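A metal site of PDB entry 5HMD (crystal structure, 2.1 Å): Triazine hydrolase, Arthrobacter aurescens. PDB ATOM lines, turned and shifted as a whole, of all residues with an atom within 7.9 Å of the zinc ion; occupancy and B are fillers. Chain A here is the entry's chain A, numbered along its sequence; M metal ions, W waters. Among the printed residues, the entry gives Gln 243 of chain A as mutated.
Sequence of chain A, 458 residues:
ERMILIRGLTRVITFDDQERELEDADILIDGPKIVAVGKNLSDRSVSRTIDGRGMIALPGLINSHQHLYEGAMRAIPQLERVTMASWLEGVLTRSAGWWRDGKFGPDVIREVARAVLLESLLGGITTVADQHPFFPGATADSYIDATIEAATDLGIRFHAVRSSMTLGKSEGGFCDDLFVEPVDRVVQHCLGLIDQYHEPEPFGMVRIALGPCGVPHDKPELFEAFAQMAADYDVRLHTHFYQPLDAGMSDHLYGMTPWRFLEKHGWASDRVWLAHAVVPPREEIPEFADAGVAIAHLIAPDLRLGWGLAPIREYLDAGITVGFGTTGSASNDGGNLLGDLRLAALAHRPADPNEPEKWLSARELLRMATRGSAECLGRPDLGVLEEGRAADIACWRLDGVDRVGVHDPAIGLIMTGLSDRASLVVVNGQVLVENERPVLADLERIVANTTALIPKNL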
ATOM      1  N   HIS A  65      -1.627 -26.614 -20.192  1.00  0.00           N
ATOM      2  CA  HIS A  65      -1.519 -25.243 -20.630  1.00  0.00           C
ATOM      3  C   HIS A  65      -2.172 -24.260 -19.671  1.00  0.00           C
ATOM      4  O   HIS A  65      -3.407 -24.151 -19.578  1.00  0.00           O
ATOM      5  CB  HIS A  65      -2.108 -25.160 -22.024  1.00  0.00           C
ATOM      6  CG  HIS A  65      -1.836 -23.874 -22.724  1.00  0.00           C
ATOM      7  ND1 HIS A  65      -0.792 -23.716 -23.594  1.00  0.00           N
ATOM      8  CD2 HIS A  65      -2.512 -22.705 -22.713  1.00  0.00           C
ATOM      9  CE1 HIS A  65      -0.817 -22.495 -24.089  1.00  0.00           C
ATOM     10  NE2 HIS A  65      -1.847 -21.863 -23.569  1.00  0.00           N
ATOM     11  N   GLN A  66      -1.310 -23.585 -18.932  1.00  0.00           N
ATOM     12  CA  GLN A  66      -1.680 -22.545 -17.971  1.00  0.00           C
ATOM     13  C   GLN A  66      -0.926 -21.242 -18.261  1.00  0.00           C
ATOM     14  O   GLN A  66       0.086 -21.235 -18.961  1.00  0.00           O
ATOM     15  CB  GLN A  66      -1.356 -22.972 -16.543  1.00  0.00           C
ATOM     16  CG  GLN A  66      -2.553 -23.392 -15.701  1.00  0.00           C
ATOM     17  CD  GLN A  66      -3.444 -22.243 -15.349  1.00  0.00           C
ATOM     18  OE1 GLN A  66      -3.239 -21.111 -15.801  1.00  0.00           O
ATOM     19  NE2 GLN A  66      -4.475 -22.517 -14.572  1.00  0.00           N
ATOM     20  N   HIS A  67      -1.449 -20.161 -17.696  1.00  0.00           N
ATOM     21  CA  HIS A  67      -0.738 -18.895 -17.551  1.00  0.00           C
ATOM     22  C   HIS A  67      -1.073 -18.413 -16.153  1.00  0.00           C
ATOM     23  O   HIS A  67      -2.088 -17.721 -15.957  1.00  0.00           O
ATOM     24  CB  HIS A  67      -1.148 -17.825 -18.577  1.00  0.00           C
ATOM     25  CG  HIS A  67      -1.066 -18.265 -19.999  1.00  0.00           C
ATOM     26  ND1 HIS A  67       0.136 -18.546 -20.626  1.00  0.00           N
ATOM     27  CD2 HIS A  67      -2.021 -18.454 -20.916  1.00  0.00           C
ATOM     28  CE1 HIS A  67      -0.104 -18.912 -21.869  1.00  0.00           C
ATOM     29  NE2 HIS A  67      -1.409 -18.853 -22.069  1.00  0.00           N
ATOM     30  N   GLU A  70      -2.196 -14.878 -14.824  1.00  0.00           N
ATOM     31  CA  GLU A  70      -3.533 -14.361 -15.135  1.00  0.00           C
ATOM     32  C   GLU A  70      -4.566 -14.605 -14.022  1.00  0.00           C
ATOM     33  O   GLU A  70      -5.680 -14.103 -14.082  1.00  0.00           O
ATOM     34  CB  GLU A  70      -4.065 -14.968 -16.426  1.00  0.00           C
ATOM     35  CG  GLU A  70      -3.296 -14.595 -17.683  1.00  0.00           C
ATOM     36  CD  GLU A  70      -3.934 -15.208 -18.953  1.00  0.00           C
ATOM     37  OE1 GLU A  70      -5.089 -15.714 -18.896  1.00  0.00           O
ATOM     38  OE2 GLU A  70      -3.299 -15.173 -20.015  1.00  0.00           O
ATOM     39  N   MET A  84     -10.600 -11.844 -29.565  1.00  0.00           N
ATOM     40  CA  MET A  84      -9.165 -12.029 -29.327  1.00  0.00           C
ATOM     41  C   MET A  84      -8.396 -10.711 -29.320  1.00  0.00           C
ATOM     42  O   MET A  84      -7.612 -10.447 -28.410  1.00  0.00           O
ATOM     43  CB  MET A  84      -8.561 -12.968 -30.363  1.00  0.00           C
ATOM     44  CG  MET A  84      -7.082 -13.252 -30.159  1.00  0.00           C
ATOM     45  SD  MET A  84      -6.660 -13.470 -28.422  1.00  0.00           S
ATOM     46  CE  MET A  84      -5.598 -14.914 -28.511  1.00  0.00           C
ATOM     47  N   TRP A  87      -9.155  -8.672 -26.307  1.00  0.00           N
ATOM     48  CA  TRP A  87      -8.739  -9.435 -25.122  1.00  0.00           C
ATOM     49  C   TRP A  87      -7.239  -9.314 -25.008  1.00  0.00           C
ATOM     50  O   TRP A  87      -6.720  -9.049 -23.940  1.00  0.00           O
ATOM     51  CB  TRP A  87      -9.163 -10.918 -25.214  1.00  0.00           C
ATOM     52  CG  TRP A  87      -8.726 -11.794 -24.051  1.00  0.00           C
ATOM     53  CD1 TRP A  87      -9.437 -12.074 -22.906  1.00  0.00           C
ATOM     54  CD2 TRP A  87      -7.504 -12.541 -23.957  1.00  0.00           C
ATOM     55  NE1 TRP A  87      -8.711 -12.925 -22.097  1.00  0.00           N
ATOM     56  CE2 TRP A  87      -7.523 -13.223 -22.713  1.00  0.00           C
ATOM     57  CE3 TRP A  87      -6.393 -12.689 -24.782  1.00  0.00           C
ATOM     58  CZ2 TRP A  87      -6.469 -14.039 -22.285  1.00  0.00           C
ATOM     59  CZ3 TRP A  87      -5.335 -13.496 -24.354  1.00  0.00           C
ATOM     60  CH2 TRP A  87      -5.395 -14.162 -23.120  1.00  0.00           C
ATOM     61  N   GLN A 131       3.028 -21.510 -18.972  1.00  0.00           N
ATOM     62  CA  GLN A 131       3.684 -20.726 -20.001  1.00  0.00           C
ATOM     63  C   GLN A 131       3.680 -19.246 -19.616  1.00  0.00           C
ATOM     64  O   GLN A 131       2.653 -18.572 -19.699  1.00  0.00           O
ATOM     65  CB  GLN A 131       2.980 -20.925 -21.330  1.00  0.00           C
ATOM     66  CG  GLN A 131       3.796 -20.520 -22.530  1.00  0.00           C
ATOM     67  CD  GLN A 131       3.107 -20.811 -23.845  1.00  0.00           C
ATOM     68  OE1 GLN A 131       1.875 -21.025 -23.894  1.00  0.00           O
ATOM     69  NE2 GLN A 131       3.874 -20.824 -24.921  1.00  0.00           N
ATOM     70  N   SER A 163       8.150 -18.372 -22.181  1.00  0.00           N
ATOM     71  CA  SER A 163       7.507 -17.845 -23.375  1.00  0.00           C
ATOM     72  C   SER A 163       8.055 -16.465 -23.684  1.00  0.00           C
ATOM     73  O   SER A 163       8.947 -15.959 -22.977  1.00  0.00           O
ATOM     74  CB  SER A 163       5.972 -17.854 -23.228  1.00  0.00           C
ATOM     75  OG  SER A 163       5.329 -17.549 -24.455  1.00  0.00           O
ATOM     76  N   CYS A 213       5.139 -17.547 -27.932  1.00  0.00           N
ATOM     77  CA  CYS A 213       3.703 -17.330 -27.876  1.00  0.00           C
ATOM     78  C   CYS A 213       3.049 -17.894 -29.146  1.00  0.00           C
ATOM     79  O   CYS A 213       2.039 -18.582 -29.083  1.00  0.00           O
ATOM     80  CB  CYS A 213       3.364 -15.838 -27.710  1.00  0.00           C
ATOM     81  SG  CYS A 213       1.611 -15.424 -28.013  1.00  0.00           S
ATOM     82  N   HIS A 238       6.770 -25.878 -27.166  1.00  0.00           N
ATOM     83  CA  HIS A 238       5.369 -25.615 -27.038  1.00  0.00           C
ATOM     84  C   HIS A 238       4.991 -24.308 -27.665  1.00  0.00           C
ATOM     85  O   HIS A 238       5.714 -23.325 -27.512  1.00  0.00           O
ATOM     86  CB  HIS A 238       4.983 -25.611 -25.566  1.00  0.00           C
ATOM     87  CG  HIS A 238       3.515 -25.492 -25.332  1.00  0.00           C
ATOM     88  ND1 HIS A 238       2.593 -26.244 -26.029  1.00  0.00           N
ATOM     89  CD2 HIS A 238       2.805 -24.714 -24.485  1.00  0.00           C
ATOM     90  CE1 HIS A 238       1.380 -25.933 -25.612  1.00  0.00           C
ATOM     91  NE2 HIS A 238       1.483 -25.012 -24.682  1.00  0.00           N
ATOM     92  N   THR A 239       3.866 -24.268 -28.368  1.00  0.00           N
ATOM     93  CA  THR A 239       3.340 -22.975 -28.791  1.00  0.00           C
ATOM     94  C   THR A 239       1.846 -23.063 -29.098  1.00  0.00           C
ATOM     95  O   THR A 239       1.301 -24.172 -29.151  1.00  0.00           O
ATOM     96  CB  THR A 239       4.103 -22.451 -30.024  1.00  0.00           C
ATOM     97  OG1 THR A 239       3.758 -21.068 -30.244  1.00  0.00           O
ATOM     98  CG2 THR A 239       3.813 -23.281 -31.253  1.00  0.00           C
ATOM     99  N   HIS A 240       1.195 -21.912 -29.259  1.00  0.00           N
ATOM    100  CA  HIS A 240      -0.183 -21.852 -29.702  1.00  0.00           C
ATOM    101  C   HIS A 240      -0.255 -22.188 -31.181  1.00  0.00           C
ATOM    102  O   HIS A 240       0.718 -22.057 -31.906  1.00  0.00           O
ATOM    103  CB  HIS A 240      -0.794 -20.479 -29.457  1.00  0.00           C
ATOM    104  CG  HIS A 240      -0.788 -20.052 -28.013  1.00  0.00           C
ATOM    105  ND1 HIS A 240       0.303 -19.474 -27.397  1.00  0.00           N
ATOM    106  CD2 HIS A 240      -1.754 -20.105 -27.071  1.00  0.00           C
ATOM    107  CE1 HIS A 240       0.019 -19.214 -26.136  1.00  0.00           C
ATOM    108  NE2 HIS A 240      -1.225 -19.593 -25.918  1.00  0.00           N
ATOM    109  N   GLN A 243      -5.175 -20.700 -33.836  1.00  0.00           N
ATOM    110  CA  GLN A 243      -6.190 -19.736 -33.414  1.00  0.00           C
ATOM    111  C   GLN A 243      -6.722 -19.051 -34.689  1.00  0.00           C
ATOM    112  O   GLN A 243      -5.952 -18.767 -35.608  1.00  0.00           O
ATOM    113  CB  GLN A 243      -5.592 -18.757 -32.422  1.00  0.00           C
ATOM    114  CG  GLN A 243      -5.112 -19.485 -31.163  1.00  0.00           C
ATOM    115  CD  GLN A 243      -4.502 -18.568 -30.120  1.00  0.00           C
ATOM    116  OE1 GLN A 243      -4.454 -18.917 -28.944  1.00  0.00           O
ATOM    117  NE2 GLN A 243      -4.000 -17.419 -30.548  1.00  0.00           N
ATOM    118  N   ALA A 275      -0.964 -25.797 -28.487  1.00  0.00           N
ATOM    119  CA  ALA A 275      -2.174 -25.348 -27.782  1.00  0.00           C
ATOM    120  C   ALA A 275      -3.347 -24.911 -28.705  1.00  0.00           C
ATOM    121  O   ALA A 275      -3.150 -24.177 -29.668  1.00  0.00           O
ATOM    122  CB  ALA A 275      -1.809 -24.195 -26.830  1.00  0.00           C
ATOM    123  N   HIS A 276      -4.551 -25.368 -28.352  1.00  0.00           N
ATOM    124  CA  HIS A 276      -5.823 -25.052 -29.026  1.00  0.00           C
ATOM    125  C   HIS A 276      -6.030 -25.898 -30.295  1.00  0.00           C
ATOM    126  O   HIS A 276      -6.895 -26.804 -30.346  1.00  0.00           O
ATOM    127  CB  HIS A 276      -5.952 -23.566 -29.399  1.00  0.00           C
ATOM    128  CG  HIS A 276      -5.787 -22.632 -28.243  1.00  0.00           C
ATOM    129  ND1 HIS A 276      -6.817 -22.302 -27.396  1.00  0.00           N
ATOM    130  CD2 HIS A 276      -4.708 -21.918 -27.820  1.00  0.00           C
ATOM    131  CE1 HIS A 276      -6.382 -21.450 -26.482  1.00  0.00           C
ATOM    132  NE2 HIS A 276      -5.110 -21.198 -26.714  1.00  0.00           N
ATOM    133  N   LEU A 298      -8.185 -27.133 -25.429  1.00  0.00           N
ATOM    134  CA  LEU A 298      -8.465 -26.051 -24.470  1.00  0.00           C
ATOM    135  C   LEU A 298      -9.884 -25.493 -24.645  1.00  0.00           C
ATOM    136  O   LEU A 298     -10.047 -24.401 -25.162  1.00  0.00           O
ATOM    137  CB  LEU A 298      -7.458 -24.935 -24.665  1.00  0.00           C
ATOM    138  CG  LEU A 298      -6.006 -25.390 -24.759  1.00  0.00           C
ATOM    139  CD1 LEU A 298      -5.053 -24.196 -25.014  1.00  0.00           C
ATOM    140  CD2 LEU A 298      -5.608 -26.151 -23.520  1.00  0.00           C
ATOM    141  N   PRO A 301     -11.341 -21.524 -23.173  1.00  0.00           N
ATOM    142  CA  PRO A 301     -11.064 -20.298 -23.945  1.00  0.00           C
ATOM    143  C   PRO A 301     -11.556 -20.332 -25.397  1.00  0.00           C
ATOM    144  O   PRO A 301     -11.862 -19.270 -25.961  1.00  0.00           O
ATOM    145  CB  PRO A 301      -9.528 -20.207 -23.904  1.00  0.00           C
ATOM    146  CG  PRO A 301      -9.065 -21.591 -23.688  1.00  0.00           C
ATOM    147  CD  PRO A 301     -10.099 -22.214 -22.786  1.00  0.00           C
ATOM    148  N   TRP A 307     -14.264 -18.749 -30.613  1.00  0.00           N
ATOM    149  CA  TRP A 307     -13.502 -19.481 -31.619  1.00  0.00           C
ATOM    150  C   TRP A 307     -14.205 -20.761 -32.057  1.00  0.00           C
ATOM    151  O   TRP A 307     -14.101 -21.142 -33.217  1.00  0.00           O
ATOM    152  CB  TRP A 307     -12.124 -19.827 -31.084  1.00  0.00           C
ATOM    153  CG  TRP A 307     -11.254 -18.666 -30.894  1.00  0.00           C
ATOM    154  CD1 TRP A 307     -11.465 -17.390 -31.343  1.00  0.00           C
ATOM    155  CD2 TRP A 307      -9.996 -18.657 -30.211  1.00  0.00           C
ATOM    156  NE1 TRP A 307     -10.399 -16.591 -30.999  1.00  0.00           N
ATOM    157  CE2 TRP A 307      -9.490 -17.342 -30.294  1.00  0.00           C
ATOM    158  CE3 TRP A 307      -9.242 -19.636 -29.540  1.00  0.00           C
ATOM    159  CZ2 TRP A 307      -8.277 -16.978 -29.714  1.00  0.00           C
ATOM    160  CZ3 TRP A 307      -8.041 -19.266 -28.977  1.00  0.00           C
ATOM    161  CH2 TRP A 307      -7.563 -17.962 -29.067  1.00  0.00           C
ATOM    162  N   THR A 326      -6.673 -25.691 -19.275  1.00  0.00           N
ATOM    163  CA  THR A 326      -7.617 -24.651 -18.939  1.00  0.00           C
ATOM    164  C   THR A 326      -7.273 -23.340 -19.609  1.00  0.00           C
ATOM    165  O   THR A 326      -8.086 -22.588 -19.941  1.00  0.00           O
ATOM    166  CB  THR A 326      -7.663 -24.443 -17.445  1.00  0.00           C
ATOM    167  OG1 THR A 326      -6.377 -24.164 -16.934  1.00  0.00           O
ATOM    168  CG2 THR A 326      -8.279 -25.600 -16.769  1.00  0.00           C
ATOM    169  N   THR A 327      -5.983 -23.150 -19.813  1.00  0.00           N
ATOM    170  CA  THR A 327      -5.363 -21.917 -20.231  1.00  0.00           C
ATOM    171  C   THR A 327      -5.328 -20.959 -19.024  1.00  0.00           C
ATOM    172  O   THR A 327      -5.730 -21.323 -18.006  1.00  0.00           O
ATOM    173  CB  THR A 327      -5.981 -21.326 -21.544  1.00  0.00           C
ATOM    174  OG1 THR A 327      -4.960 -20.820 -22.379  1.00  0.00           O
ATOM    175  CG2 THR A 327      -6.920 -20.271 -21.290  1.00  0.00           C
ATOM    176  N   GLY A 328      -4.824 -19.768 -19.157  1.00  0.00           N
ATOM    177  CA  GLY A 328      -4.839 -18.806 -18.063  1.00  0.00           C
ATOM    178  C   GLY A 328      -6.246 -18.349 -17.627  1.00  0.00           C
ATOM    179  O   GLY A 328      -7.228 -18.455 -18.380  1.00  0.00           O
ATOM    180  N   SER A 331      -8.832 -15.923 -19.474  1.00  0.00           N
ATOM    181  CA  SER A 331      -9.707 -16.466 -20.489  1.00  0.00           C
ATOM    182  C   SER A 331     -10.168 -17.850 -20.136  1.00  0.00           C
ATOM    183  O   SER A 331      -9.992 -18.787 -20.929  1.00  0.00           O
ATOM    184  CB  SER A 331      -9.007 -16.499 -21.843  1.00  0.00           C
ATOM    185  OG  SER A 331      -7.935 -17.431 -21.828  1.00  0.00           O
HETATM  186 ZN    ZN M   1      -2.204 -19.707 -23.920  1.00  0.00          ZN
HETATM  187  O   HOH W   1      -4.385 -19.038 -24.542  1.00  0.00           O
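Water W1 lies within hydrogen-bond range of the side-chain hydroxyl (OG1) of Thr 327 (2.9 Å) and a ring nitrogen (NE2) of His 276 (3.1 Å).
The backbone carbonyl oxygen of His 65 lies within hydrogen-bond range of the backbone NH of Thr 327, 2.8 Å away.
A ring nitrogen (ND1) of His 67 lies within hydrogen-bond range of the backbone carbonyl oxygen (O) of Gln 131 (2.7 Å).
The backbone carbonyl oxygen (O) of Thr 327 sits close to the side-chain amide oxygen (OE1) of Gln 66 (3.3 Å).
ND1 of His 65 is in hydrogen-bond range of NE2 of His 238 (2.8 Å).
O of Cys 213 lies within hydrogen-bond range of ND1 of His 240 (2.6 Å).
The zinc ion is bound by NE2 of His 67 (2.2 Å), NE2 of His 65 (2.2 Å), NE2 of His 240 (2.2 Å) and water W1 (2.4 Å).
Residues that only touch the zinc ion: Thr 327.
Within 4 Å of the zinc ion: His 65, His 67, His 240 and Thr 327.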
